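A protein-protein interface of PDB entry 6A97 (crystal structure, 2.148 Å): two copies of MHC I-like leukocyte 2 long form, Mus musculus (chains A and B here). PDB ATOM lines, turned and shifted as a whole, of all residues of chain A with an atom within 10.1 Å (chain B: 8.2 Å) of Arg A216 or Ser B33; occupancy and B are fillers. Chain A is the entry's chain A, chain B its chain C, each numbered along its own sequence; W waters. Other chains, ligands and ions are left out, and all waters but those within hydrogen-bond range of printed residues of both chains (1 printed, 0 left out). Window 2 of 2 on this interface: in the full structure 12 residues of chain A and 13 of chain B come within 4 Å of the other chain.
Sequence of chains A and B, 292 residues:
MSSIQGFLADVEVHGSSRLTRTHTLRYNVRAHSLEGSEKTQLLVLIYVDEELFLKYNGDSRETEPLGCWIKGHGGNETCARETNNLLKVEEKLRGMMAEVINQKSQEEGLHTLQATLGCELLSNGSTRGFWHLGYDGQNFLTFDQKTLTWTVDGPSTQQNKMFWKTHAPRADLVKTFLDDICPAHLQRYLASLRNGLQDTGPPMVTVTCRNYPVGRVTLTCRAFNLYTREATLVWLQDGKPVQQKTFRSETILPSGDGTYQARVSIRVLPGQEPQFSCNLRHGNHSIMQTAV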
ATOM      1  N   CYS A 209      22.039   7.499 -16.345  1.00  0.00           N
ATOM      2  CA  CYS A 209      22.374   8.849 -16.772  1.00  0.00           C
ATOM      3  C   CYS A 209      23.658   9.307 -16.094  1.00  0.00           C
ATOM      4  O   CYS A 209      23.913   8.967 -14.940  1.00  0.00           O
ATOM      5  CB  CYS A 209      21.234   9.820 -16.444  1.00  0.00           C
ATOM      6  SG  CYS A 209      19.578   9.220 -16.862  1.00  0.00           S
ATOM      7  N   ARG A 210      24.465  10.076 -16.816  1.00  0.00           N
ATOM      8  CA  ARG A 210      25.656  10.677 -16.234  1.00  0.00           C
ATOM      9  C   ARG A 210      25.862  12.093 -16.768  1.00  0.00           C
ATOM     10  O   ARG A 210      25.773  12.332 -17.972  1.00  0.00           O
ATOM     11  CB  ARG A 210      26.892   9.817 -16.513  1.00  0.00           C
ATOM     12  CG  ARG A 210      28.186  10.459 -16.040  1.00  0.00           C
ATOM     13  CD  ARG A 210      29.397   9.571 -16.270  1.00  0.00           C
ATOM     14  NE  ARG A 210      30.329   9.646 -15.148  1.00  0.00           N
ATOM     15  CZ  ARG A 210      31.650   9.713 -15.272  1.00  0.00           C
ATOM     16  NH1 ARG A 210      32.418   9.780 -14.192  1.00  0.00           N
ATOM     17  NH2 ARG A 210      32.206   9.718 -16.477  1.00  0.00           N
ATOM     18  N   ASN A 211      26.132  13.030 -15.866  1.00  0.00           N
ATOM     19  CA  ASN A 211      26.418  14.404 -16.263  1.00  0.00           C
ATOM     20  C   ASN A 211      27.802  14.510 -16.894  1.00  0.00           C
ATOM     21  O   ASN A 211      28.745  15.003 -16.278  1.00  0.00           O
ATOM     22  CB  ASN A 211      26.304  15.342 -15.061  1.00  0.00           C
ATOM     23  CG  ASN A 211      24.889  15.424 -14.523  1.00  0.00           C
ATOM     24  OD1 ASN A 211      23.926  15.452 -15.288  1.00  0.00           O
ATOM     25  ND2 ASN A 211      24.756  15.467 -13.203  1.00  0.00           N
ATOM     26  N   TYR A 212      27.911  14.038 -18.132  1.00  0.00           N
ATOM     27  CA  TYR A 212      29.186  13.973 -18.833  1.00  0.00           C
ATOM     28  C   TYR A 212      28.948  13.831 -20.334  1.00  0.00           C
ATOM     29  O   TYR A 212      28.059  13.088 -20.751  1.00  0.00           O
ATOM     30  CB  TYR A 212      30.024  12.801 -18.312  1.00  0.00           C
ATOM     31  CG  TYR A 212      31.409  12.700 -18.917  1.00  0.00           C
ATOM     32  CD1 TYR A 212      31.639  11.937 -20.056  1.00  0.00           C
ATOM     33  CD2 TYR A 212      32.487  13.366 -18.345  1.00  0.00           C
ATOM     34  CE1 TYR A 212      32.905  11.842 -20.611  1.00  0.00           C
ATOM     35  CE2 TYR A 212      33.757  13.279 -18.892  1.00  0.00           C
ATOM     36  CZ  TYR A 212      33.959  12.515 -20.024  1.00  0.00           C
ATOM     37  OH  TYR A 212      35.218  12.423 -20.573  1.00  0.00           O
ATOM     38  N   PRO A 213      29.733  14.550 -21.154  1.00  0.00           N
ATOM     39  CA  PRO A 213      30.733  15.547 -20.747  1.00  0.00           C
ATOM     40  C   PRO A 213      30.125  16.861 -20.246  1.00  0.00           C
ATOM     41  O   PRO A 213      28.922  16.921 -19.993  1.00  0.00           O
ATOM     42  CB  PRO A 213      31.546  15.775 -22.027  1.00  0.00           C
ATOM     43  CG  PRO A 213      30.649  15.351 -23.135  1.00  0.00           C
ATOM     44  CD  PRO A 213      29.820  14.234 -22.590  1.00  0.00           C
ATOM     45  N   VAL A 214      30.969  17.887 -20.134  1.00  0.00           N
ATOM     46  CA  VAL A 214      30.686  19.125 -19.397  1.00  0.00           C
ATOM     47  C   VAL A 214      29.242  19.639 -19.432  1.00  0.00           C
ATOM     48  O   VAL A 214      28.604  19.776 -18.387  1.00  0.00           O
ATOM     49  CB  VAL A 214      31.601  20.266 -19.895  1.00  0.00           C
ATOM     50  CG1 VAL A 214      31.268  21.568 -19.183  1.00  0.00           C
ATOM     51  CG2 VAL A 214      33.066  19.898 -19.692  1.00  0.00           C
ATOM     52  N   GLY A 215      28.728  19.931 -20.619  1.00  0.00           N
ATOM     53  CA  GLY A 215      27.391  20.491 -20.729  1.00  0.00           C
ATOM     54  C   GLY A 215      26.364  19.495 -21.232  1.00  0.00           C
ATOM     55  O   GLY A 215      25.345  19.876 -21.807  1.00  0.00           O
ATOM     56  N   ARG A 216      26.631  18.212 -21.015  1.00  0.00           N
ATOM     57  CA  ARG A 216      25.773  17.162 -21.545  1.00  0.00           C
ATOM     58  C   ARG A 216      25.367  16.139 -20.494  1.00  0.00           C
ATOM     59  O   ARG A 216      25.927  16.089 -19.398  1.00  0.00           O
ATOM     60  CB  ARG A 216      26.474  16.433 -22.695  1.00  0.00           C
ATOM     61  CG  ARG A 216      26.968  17.329 -23.809  1.00  0.00           C
ATOM     62  CD  ARG A 216      25.828  17.806 -24.684  1.00  0.00           C
ATOM     63  NE  ARG A 216      26.329  18.550 -25.835  1.00  0.00           N
ATOM     64  CZ  ARG A 216      26.565  19.857 -25.835  1.00  0.00           C
ATOM     65  NH1 ARG A 216      26.339  20.578 -24.742  1.00  0.00           N
ATOM     66  NH2 ARG A 216      27.026  20.444 -26.931  1.00  0.00           N
ATOM     67  N   VAL A 217      24.388  15.319 -20.850  1.00  0.00           N
ATOM     68  CA  VAL A 217      24.050  14.141 -20.074  1.00  0.00           C
ATOM     69  C   VAL A 217      24.167  12.931 -20.981  1.00  0.00           C
ATOM     70  O   VAL A 217      23.515  12.870 -22.023  1.00  0.00           O
ATOM     71  CB  VAL A 217      22.627  14.213 -19.485  1.00  0.00           C
ATOM     72  CG1 VAL A 217      22.248  12.875 -18.864  1.00  0.00           C
ATOM     73  CG2 VAL A 217      22.528  15.336 -18.459  1.00  0.00           C
ATOM     74  N   THR A 218      25.006  11.977 -20.603  1.00  0.00           N
ATOM     75  CA  THR A 218      25.131  10.751 -21.376  1.00  0.00           C
ATOM     76  C   THR A 218      24.106   9.728 -20.900  1.00  0.00           C
ATOM     77  O   THR A 218      24.127   9.306 -19.742  1.00  0.00           O
ATOM     78  CB  THR A 218      26.547  10.156 -21.277  1.00  0.00           C
ATOM     79  OG1 THR A 218      27.494  11.082 -21.826  1.00  0.00           O
ATOM     80  CG2 THR A 218      26.634   8.845 -22.043  1.00  0.00           C
ATOM     81  N   LEU A 219      23.193   9.356 -21.791  1.00  0.00           N
ATOM     82  CA  LEU A 219      22.205   8.325 -21.502  1.00  0.00           C
ATOM     83  C   LEU A 219      22.721   6.986 -21.993  1.00  0.00           C
ATOM     84  O   LEU A 219      23.059   6.844 -23.166  1.00  0.00           O
ATOM     85  CB  LEU A 219      20.863   8.643 -22.167  1.00  0.00           C
ATOM     86  CG  LEU A 219      20.198   9.970 -21.796  1.00  0.00           C
ATOM     87  CD1 LEU A 219      18.937  10.197 -22.631  1.00  0.00           C
ATOM     88  CD2 LEU A 219      19.871  10.006 -20.320  1.00  0.00           C
ATOM     89  N   ILE A 266      23.929   7.751 -25.904  1.00  0.00           N
ATOM     90  CA  ILE A 266      23.761   9.007 -26.629  1.00  0.00           C
ATOM     91  C   ILE A 266      24.023  10.166 -25.683  1.00  0.00           C
ATOM     92  O   ILE A 266      23.967  10.002 -24.464  1.00  0.00           O
ATOM     93  CB  ILE A 266      22.345   9.167 -27.225  1.00  0.00           C
ATOM     94  CG1 ILE A 266      21.288   9.038 -26.125  1.00  0.00           C
ATOM     95  CG2 ILE A 266      22.101   8.142 -28.335  1.00  0.00           C
ATOM     96  CD1 ILE A 266      19.870   9.285 -26.599  1.00  0.00           C
ATOM     97  N   ARG A 267      24.305  11.336 -26.245  1.00  0.00           N
ATOM     98  CA  ARG A 267      24.477  12.536 -25.441  1.00  0.00           C
ATOM     99  C   ARG A 267      23.350  13.510 -25.731  1.00  0.00           C
ATOM    100  O   ARG A 267      23.042  13.794 -26.888  1.00  0.00           O
ATOM    101  CB  ARG A 267      25.836  13.185 -25.709  1.00  0.00           C
ATOM    102  CG  ARG A 267      27.000  12.362 -25.190  1.00  0.00           C
ATOM    103  CD  ARG A 267      28.101  12.251 -26.221  1.00  0.00           C
ATOM    104  NE  ARG A 267      28.645  10.897 -26.267  1.00  0.00           N
ATOM    105  CZ  ARG A 267      28.095   9.897 -26.950  1.00  0.00           C
ATOM    106  NH1 ARG A 267      26.986  10.099 -27.648  1.00  0.00           N
ATOM    107  NH2 ARG A 267      28.654   8.698 -26.938  1.00  0.00           N
ATOM    108  N   VAL A 268      22.718  13.999 -24.670  1.00  0.00           N
ATOM    109  CA  VAL A 268      21.631  14.952 -24.804  1.00  0.00           C
ATOM    110  C   VAL A 268      21.919  16.135 -23.908  1.00  0.00           C
ATOM    111  O   VAL A 268      22.871  16.108 -23.127  1.00  0.00           O
ATOM    112  CB  VAL A 268      20.271  14.328 -24.432  1.00  0.00           C
ATOM    113  CG1 VAL A 268      20.068  13.034 -25.191  1.00  0.00           C
ATOM    114  CG2 VAL A 268      20.185  14.084 -22.929  1.00  0.00           C
ATOM    115  N   LEU A 269      21.103  17.175 -24.029  1.00  0.00           N
ATOM    116  CA  LEU A 269      21.231  18.353 -23.185  1.00  0.00           C
ATOM    117  C   LEU A 269      20.504  18.142 -21.860  1.00  0.00           C
ATOM    118  O   LEU A 269      19.504  17.425 -21.810  1.00  0.00           O
ATOM    119  CB  LEU A 269      20.683  19.587 -23.904  1.00  0.00           C
ATOM    120  CG  LEU A 269      21.287  19.879 -25.278  1.00  0.00           C
ATOM    121  CD1 LEU A 269      20.576  21.050 -25.935  1.00  0.00           C
ATOM    122  CD2 LEU A 269      22.784  20.147 -25.160  1.00  0.00           C
ATOM    123  N   PRO A 270      21.012  18.757 -20.780  1.00  0.00           N
ATOM    124  CA  PRO A 270      20.391  18.662 -19.453  1.00  0.00           C
ATOM    125  C   PRO A 270      18.904  19.011 -19.479  1.00  0.00           C
ATOM    126  O   PRO A 270      18.527  20.059 -20.003  1.00  0.00           O
ATOM    127  CB  PRO A 270      21.177  19.684 -18.627  1.00  0.00           C
ATOM    128  CG  PRO A 270      22.515  19.734 -19.278  1.00  0.00           C
ATOM    129  CD  PRO A 270      22.264  19.537 -20.749  1.00  0.00           C
ATOM    130  N   GLY A 271      18.073  18.133 -18.933  1.00  0.00           N
ATOM    131  CA  GLY A 271      16.642  18.371 -18.892  1.00  0.00           C
ATOM    132  C   GLY A 271      15.884  17.708 -20.026  1.00  0.00           C
ATOM    133  O   GLY A 271      14.655  17.728 -20.050  1.00  0.00           O
ATOM    134  N   GLN A 272      16.611  17.118 -20.969  1.00  0.00           N
ATOM    135  CA  GLN A 272      15.986  16.488 -22.128  1.00  0.00           C
ATOM    136  C   GLN A 272      15.663  15.013 -21.913  1.00  0.00           C
ATOM    137  O   GLN A 272      14.968  14.410 -22.731  1.00  0.00           O
ATOM    138  CB  GLN A 272      16.883  16.614 -23.361  1.00  0.00           C
ATOM    139  CG  GLN A 272      16.781  17.936 -24.100  1.00  0.00           C
ATOM    140  CD  GLN A 272      17.440  17.871 -25.465  1.00  0.00           C
ATOM    141  OE1 GLN A 272      18.512  17.279 -25.624  1.00  0.00           O
ATOM    142  NE2 GLN A 272      16.796  18.469 -26.464  1.00  0.00           N
ATOM    143  N   GLU A 273      16.171  14.436 -20.823  1.00  0.00           N
ATOM    144  CA  GLU A 273      16.076  12.990 -20.589  1.00  0.00           C
ATOM    145  C   GLU A 273      14.673  12.383 -20.769  1.00  0.00           C
ATOM    146  O   GLU A 273      14.554  11.330 -21.391  1.00  0.00           O
ATOM    147  CB  GLU A 273      16.603  12.640 -19.192  1.00  0.00           C
ATOM    148  CG  GLU A 273      18.047  13.047 -18.939  1.00  0.00           C
ATOM    149  CD  GLU A 273      18.159  14.398 -18.260  1.00  0.00           C
ATOM    150  OE1 GLU A 273      17.365  15.299 -18.600  1.00  0.00           O
ATOM    151  OE2 GLU A 273      19.038  14.557 -17.385  1.00  0.00           O
ATOM    152  N   ARG B  30      17.268  24.973 -28.631  1.00  0.00           N
ATOM    153  CA  ARG B  30      18.097  25.148 -27.447  1.00  0.00           C
ATOM    154  C   ARG B  30      19.519  25.532 -27.833  1.00  0.00           C
ATOM    155  O   ARG B  30      20.122  24.899 -28.697  1.00  0.00           O
ATOM    156  CB  ARG B  30      18.112  23.870 -26.601  1.00  0.00           C
ATOM    157  CG  ARG B  30      16.865  23.676 -25.753  1.00  0.00           C
ATOM    158  CD  ARG B  30      17.073  22.626 -24.670  1.00  0.00           C
ATOM    159  NE  ARG B  30      18.052  23.046 -23.671  1.00  0.00           N
ATOM    160  CZ  ARG B  30      18.320  22.364 -22.563  1.00  0.00           C
ATOM    161  NH1 ARG B  30      17.678  21.231 -22.309  1.00  0.00           N
ATOM    162  NH2 ARG B  30      19.228  22.810 -21.704  1.00  0.00           N
ATOM    163  N   ALA B  31      20.049  26.567 -27.191  1.00  0.00           N
ATOM    164  CA  ALA B  31      21.439  26.956 -27.393  1.00  0.00           C
ATOM    165  C   ALA B  31      22.379  25.865 -26.893  1.00  0.00           C
ATOM    166  O   ALA B  31      22.077  25.168 -25.923  1.00  0.00           O
ATOM    167  CB  ALA B  31      21.734  28.277 -26.688  1.00  0.00           C
ATOM    168  N   HIS B  32      23.514  25.715 -27.568  1.00  0.00           N
ATOM    169  CA  HIS B  32      24.540  24.767 -27.154  1.00  0.00           C
ATOM    170  C   HIS B  32      25.848  25.057 -27.882  1.00  0.00           C
ATOM    171  O   HIS B  32      25.858  25.715 -28.923  1.00  0.00           O
ATOM    172  CB  HIS B  32      24.094  23.326 -27.416  1.00  0.00           C
ATOM    173  CG  HIS B  32      23.952  22.992 -28.867  1.00  0.00           C
ATOM    174  ND1 HIS B  32      24.981  22.459 -29.612  1.00  0.00           N
ATOM    175  CD2 HIS B  32      22.904  23.124 -29.713  1.00  0.00           C
ATOM    176  CE1 HIS B  32      24.570  22.270 -30.854  1.00  0.00           C
ATOM    177  NE2 HIS B  32      23.314  22.666 -30.941  1.00  0.00           N
ATOM    178  N   SER B  33      26.950  24.571 -27.323  1.00  0.00           N
ATOM    179  CA  SER B  33      28.264  24.777 -27.920  1.00  0.00           C
ATOM    180  C   SER B  33      28.755  23.518 -28.622  1.00  0.00           C
ATOM    181  O   SER B  33      28.456  22.404 -28.198  1.00  0.00           O
ATOM    182  CB  SER B  33      29.270  25.211 -26.856  1.00  0.00           C
ATOM    183  OG  SER B  33      28.761  26.294 -26.096  1.00  0.00           O
ATOM    184  N   LEU B  34      29.499  23.705 -29.706  1.00  0.00           N
ATOM    185  CA  LEU B  34      30.079  22.586 -30.436  1.00  0.00           C
ATOM    186  C   LEU B  34      31.418  22.217 -29.805  1.00  0.00           C
ATOM    187  O   LEU B  34      32.163  23.096 -29.369  1.00  0.00           O
ATOM    188  CB  LEU B  34      30.248  22.936 -31.916  1.00  0.00           C
ATOM    189  CG  LEU B  34      29.031  23.600 -32.573  1.00  0.00           C
ATOM    190  CD1 LEU B  34      29.383  24.157 -33.944  1.00  0.00           C
ATOM    191  CD2 LEU B  34      27.860  22.633 -32.665  1.00  0.00           C
ATOM    192  N   GLU B  35      31.709  20.920 -29.761  1.00  0.00           N
ATOM    193  CA  GLU B  35      32.872  20.389 -29.048  1.00  0.00           C
ATOM    194  C   GLU B  35      34.187  21.074 -29.416  1.00  0.00           C
ATOM    195  O   GLU B  35      34.937  21.494 -28.536  1.00  0.00           O
ATOM    196  CB  GLU B  35      32.997  18.883 -29.297  1.00  0.00           C
ATOM    197  N   GLY B  36      34.460  21.184 -30.711  1.00  0.00           N
ATOM    198  CA  GLY B  36      35.685  21.807 -31.184  1.00  0.00           C
ATOM    199  C   GLY B  36      35.780  23.274 -30.813  1.00  0.00           C
ATOM    200  O   GLY B  36      36.274  23.623 -29.740  1.00  0.00           O
ATOM    201  N   SER B  37      35.310  24.139 -31.706  1.00  0.00           N
ATOM    202  CA  SER B  37      35.258  25.567 -31.423  1.00  0.00           C
ATOM    203  C   SER B  37      34.056  25.871 -30.539  1.00  0.00           C
ATOM    204  O   SER B  37      32.943  25.434 -30.823  1.00  0.00           O
ATOM    205  CB  SER B  37      35.187  26.379 -32.719  1.00  0.00           C
ATOM    206  OG  SER B  37      33.991  26.103 -33.427  1.00  0.00           O
ATOM    207  N   GLU B  38      34.286  26.620 -29.467  1.00  0.00           N
ATOM    208  CA  GLU B  38      33.221  26.920 -28.519  1.00  0.00           C
ATOM    209  C   GLU B  38      32.384  28.121 -28.957  1.00  0.00           C
ATOM    210  O   GLU B  38      32.307  29.128 -28.253  1.00  0.00           O
ATOM    211  CB  GLU B  38      33.804  27.168 -27.126  1.00  0.00           C
ATOM    212  N   LYS B  39      31.765  28.011 -30.129  1.00  0.00           N
ATOM    213  CA  LYS B  39      30.770  28.985 -30.559  1.00  0.00           C
ATOM    214  C   LYS B  39      29.388  28.367 -30.405  1.00  0.00           C
ATOM    215  O   LYS B  39      29.257  27.147 -30.304  1.00  0.00           O
ATOM    216  CB  LYS B  39      31.009  29.426 -32.004  1.00  0.00           C
ATOM    217  CG  LYS B  39      32.476  29.510 -32.398  1.00  0.00           C
ATOM    218  CD  LYS B  39      32.640  30.144 -33.772  1.00  0.00           C
ATOM    219  CE  LYS B  39      31.855  29.387 -34.834  1.00  0.00           C
ATOM    220  NZ  LYS B  39      31.872  30.098 -36.146  1.00  0.00           N
ATOM    221  N   THR B  40      28.356  29.203 -30.384  1.00  0.00           N
ATOM    222  CA  THR B  40      27.010  28.724 -30.104  1.00  0.00           C
ATOM    223  C   THR B  40      26.190  28.481 -31.364  1.00  0.00           C
ATOM    224  O   THR B  40      26.193  29.289 -32.293  1.00  0.00           O
ATOM    225  CB  THR B  40      26.239  29.712 -29.208  1.00  0.00           C
ATOM    226  OG1 THR B  40      27.060  30.092 -28.099  1.00  0.00           O
ATOM    227  CG2 THR B  40      24.956  29.073 -28.692  1.00  0.00           C
ATOM    228  N   GLN B  41      25.492  27.353 -31.384  1.00  0.00           N
ATOM    229  CA  GLN B  41      24.499  27.068 -32.406  1.00  0.00           C
ATOM    230  C   GLN B  41      23.166  26.780 -31.737  1.00  0.00           C
ATOM    231  O   GLN B  41      23.078  26.709 -30.513  1.00  0.00           O
ATOM    232  CB  GLN B  41      24.916  25.876 -33.273  1.00  0.00           C
ATOM    233  CG  GLN B  41      25.972  26.190 -34.315  1.00  0.00           C
ATOM    234  CD  GLN B  41      25.963  25.200 -35.465  1.00  0.00           C
ATOM    235  OE1 GLN B  41      25.305  24.159 -35.401  1.00  0.00           O
ATOM    236  NE2 GLN B  41      26.696  25.521 -36.527  1.00  0.00           N
ATOM    237  N   LEU B  42      22.129  26.606 -32.547  1.00  0.00           N
ATOM    238  CA  LEU B  42      20.859  26.118 -32.039  1.00  0.00           C
ATOM    239  C   LEU B  42      20.645  24.664 -32.431  1.00  0.00           C
ATOM    240  O   LEU B  42      20.728  24.308 -33.605  1.00  0.00           O
ATOM    241  CB  LEU B  42      19.696  26.965 -32.554  1.00  0.00           C
ATOM    242  CG  LEU B  42      19.534  28.386 -32.013  1.00  0.00           C
ATOM    243  CD1 LEU B  42      18.327  29.056 -32.652  1.00  0.00           C
ATOM    244  CD2 LEU B  42      19.393  28.362 -30.504  1.00  0.00           C
ATOM    245  N   LEU B  43      20.399  23.822 -31.434  1.00  0.00           N
ATOM    246  CA  LEU B  43      19.796  22.523 -31.670  1.00  0.00           C
ATOM    247  C   LEU B  43      18.321  22.785 -31.929  1.00  0.00           C
ATOM    248  O   LEU B  43      17.632  23.344 -31.075  1.00  0.00           O
ATOM    249  CB  LEU B  43      19.997  21.594 -30.470  1.00  0.00           C
ATOM    250  CG  LEU B  43      19.176  20.304 -30.339  1.00  0.00           C
ATOM    251  CD1 LEU B  43      19.289  19.426 -31.568  1.00  0.00           C
ATOM    252  CD2 LEU B  43      19.612  19.531 -29.104  1.00  0.00           C
ATOM    253  N   ASN B  57      21.122  18.836 -35.169  1.00  0.00           N
ATOM    254  CA  ASN B  57      22.007  18.773 -34.014  1.00  0.00           C
ATOM    255  C   ASN B  57      23.460  18.907 -34.460  1.00  0.00           C
ATOM    256  O   ASN B  57      24.110  17.914 -34.781  1.00  0.00           O
ATOM    257  CB  ASN B  57      21.796  17.459 -33.251  1.00  0.00           C
ATOM    258  CG  ASN B  57      22.735  17.308 -32.061  1.00  0.00           C
ATOM    259  OD1 ASN B  57      23.375  18.265 -31.624  1.00  0.00           O
ATOM    260  ND2 ASN B  57      22.820  16.091 -31.534  1.00  0.00           N
ATOM    261  N   GLY B  58      23.960  20.139 -34.476  1.00  0.00           N
ATOM    262  CA  GLY B  58      25.299  20.418 -34.963  1.00  0.00           C
ATOM    263  C   GLY B  58      26.424  19.778 -34.169  1.00  0.00           C
ATOM    264  O   GLY B  58      27.545  19.665 -34.661  1.00  0.00           O
ATOM    265  N   ASP B  59      26.133  19.359 -32.941  1.00  0.00           N
ATOM    266  CA  ASP B  59      27.154  18.773 -32.081  1.00  0.00           C
ATOM    267  C   ASP B  59      26.963  17.267 -31.910  1.00  0.00           C
ATOM    268  O   ASP B  59      27.410  16.682 -30.921  1.00  0.00           O
ATOM    269  CB  ASP B  59      27.158  19.461 -30.713  1.00  0.00           C
ATOM    270  CG  ASP B  59      28.436  19.204 -29.933  1.00  0.00           C
ATOM    271  OD1 ASP B  59      29.531  19.327 -30.522  1.00  0.00           O
ATOM    272  OD2 ASP B  59      28.346  18.865 -28.733  1.00  0.00           O
ATOM    273  N   SER B  60      26.298  16.635 -32.873  1.00  0.00           N
ATOM    274  CA  SER B  60      26.173  15.181 -32.863  1.00  0.00           C
ATOM    275  C   SER B  60      27.553  14.552 -32.974  1.00  0.00           C
ATOM    276  O   SER B  60      28.481  15.165 -33.502  1.00  0.00           O
ATOM    277  CB  SER B  60      25.284  14.694 -34.005  1.00  0.00           C
ATOM    278  OG  SER B  60      25.878  14.982 -35.259  1.00  0.00           O
ATOM    279  N   ARG B  61      27.684  13.330 -32.470  1.00  0.00           N
ATOM    280  CA  ARG B  61      28.951  12.615 -32.533  1.00  0.00           C
ATOM    281  C   ARG B  61      28.789  11.303 -33.289  1.00  0.00           C
ATOM    282  O   ARG B  61      29.292  11.159 -34.402  1.00  0.00           O
ATOM    283  CB  ARG B  61      29.501  12.378 -31.124  1.00  0.00           C
ATOM    284  CG  ARG B  61      30.196  13.612 -30.563  1.00  0.00           C
ATOM    285  CD  ARG B  61      29.895  13.856 -29.094  1.00  0.00           C
ATOM    286  NE  ARG B  61      30.133  15.256 -28.744  1.00  0.00           N
ATOM    287  CZ  ARG B  61      30.262  15.714 -27.502  1.00  0.00           C
ATOM    288  NH1 ARG B  61      30.473  17.007 -27.292  1.00  0.00           N
ATOM    289  NH2 ARG B  61      30.185  14.884 -26.471  1.00  0.00           N
ATOM    290  N   THR B 112      21.964  27.755 -21.784  1.00  0.00           N
ATOM    291  CA  THR B 112      20.761  27.013 -21.423  1.00  0.00           C
ATOM    292  C   THR B 112      19.498  27.698 -21.938  1.00  0.00           C
ATOM    293  O   THR B 112      18.388  27.353 -21.534  1.00  0.00           O
ATOM    294  CB  THR B 112      20.643  26.836 -19.897  1.00  0.00           C
ATOM    295  OG1 THR B 112      20.456  28.115 -19.274  1.00  0.00           O
ATOM    296  CG2 THR B 112      21.892  26.174 -19.338  1.00  0.00           C
HETATM  297  O   HOH W   1      26.769  23.439 -24.633  1.00  0.00           O
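The backbone carbonyl oxygen (O) of Pro A270 is in hydrogen-bond range of the guanidinium group (NH1) of Arg B30 (2.7 Å). The guanidinium group (NH2) of Arg A216 is in salt-bridge range of the side-chain carboxylate (OD2) of Asp B59 (2.7 Å). O of Ser B33 lies within hydrogen-bond range of NH2 of Arg A216, at 2.7 Å.
The side-chain amide oxygen (OE1) of Gln A272 lies within hydrogen-bond range of the backbone NH (N) of Leu A269 (3.0 Å). The backbone carbonyl oxygen (O) of Arg B30 lies within hydrogen-bond range of the backbone NH (N) of Leu B43 (3.0 Å). N of Gln B41 lies within hydrogen-bond range of O of His B32 (3.0 Å). The backbone NH (N) of Leu B43 sits close to a ring nitrogen (NE2) of His B32 (3.2 Å). OD1 of Asn B57 lies close to N of Asp B59. NH1 of Arg B61 is in salt-bridge range of OD2 of Asp B59 (3.2 Å).
Among the printed residues, pairs that only touch across the chains: Pro A213 with Arg B61 (3.4 Å), Arg A216 with His B32 (3.9 Å), Arg A267 with Arg B61 (3.4 Å), Leu A269 with Arg B30 (3.8 Å), Leu A269 with Leu B43 (3.6 Å) and Gln A272 with Arg B30 (3.9 Å).
Arg A216 touches three residues of chain B. Ser B33 touches just one residue of chain A: Arg A216. His B32 touches just one residue of chain A: Arg A216. No residue of chain A comes within 4 Å of Leu B34. No residue of chain A comes within 4 Å of Glu B38. Of the printed residues of chain A, Arg B61 touches Pro A213 (3.4 Å) and Arg A267 (3.4 Å). Of the printed residues of chain B, Pro A213 touches Arg B61 (3.4 Å). The nearest residue of chain A that does not touch Ser B33 is Leu A269 (6.5 Å). The nearest printed residue of chain B that does not touch Leu A269 is His B32 (4.1 Å).
Hydrophobic or aromatic side chains of chain B that line the printed part of chain A: His B32 and Leu B43. Hydrophobic or aromatic side chains of chain A that line the printed part of chain B: Pro A213 and Leu A269. Among the printed residues, 9 pairs touch across the chains. Among the printed residues, Asp or Glu carboxylates within 4 Å of a Lys or Arg side-chain nitrogen of the other chain: Arg A216 with Asp B59.
No position is printed for both chains.
Water W1 bridges the guanidinium group (NH1) of Arg A216 (2.9 Å) and the backbone NH (N) of Ser B33 (2.9 Å).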
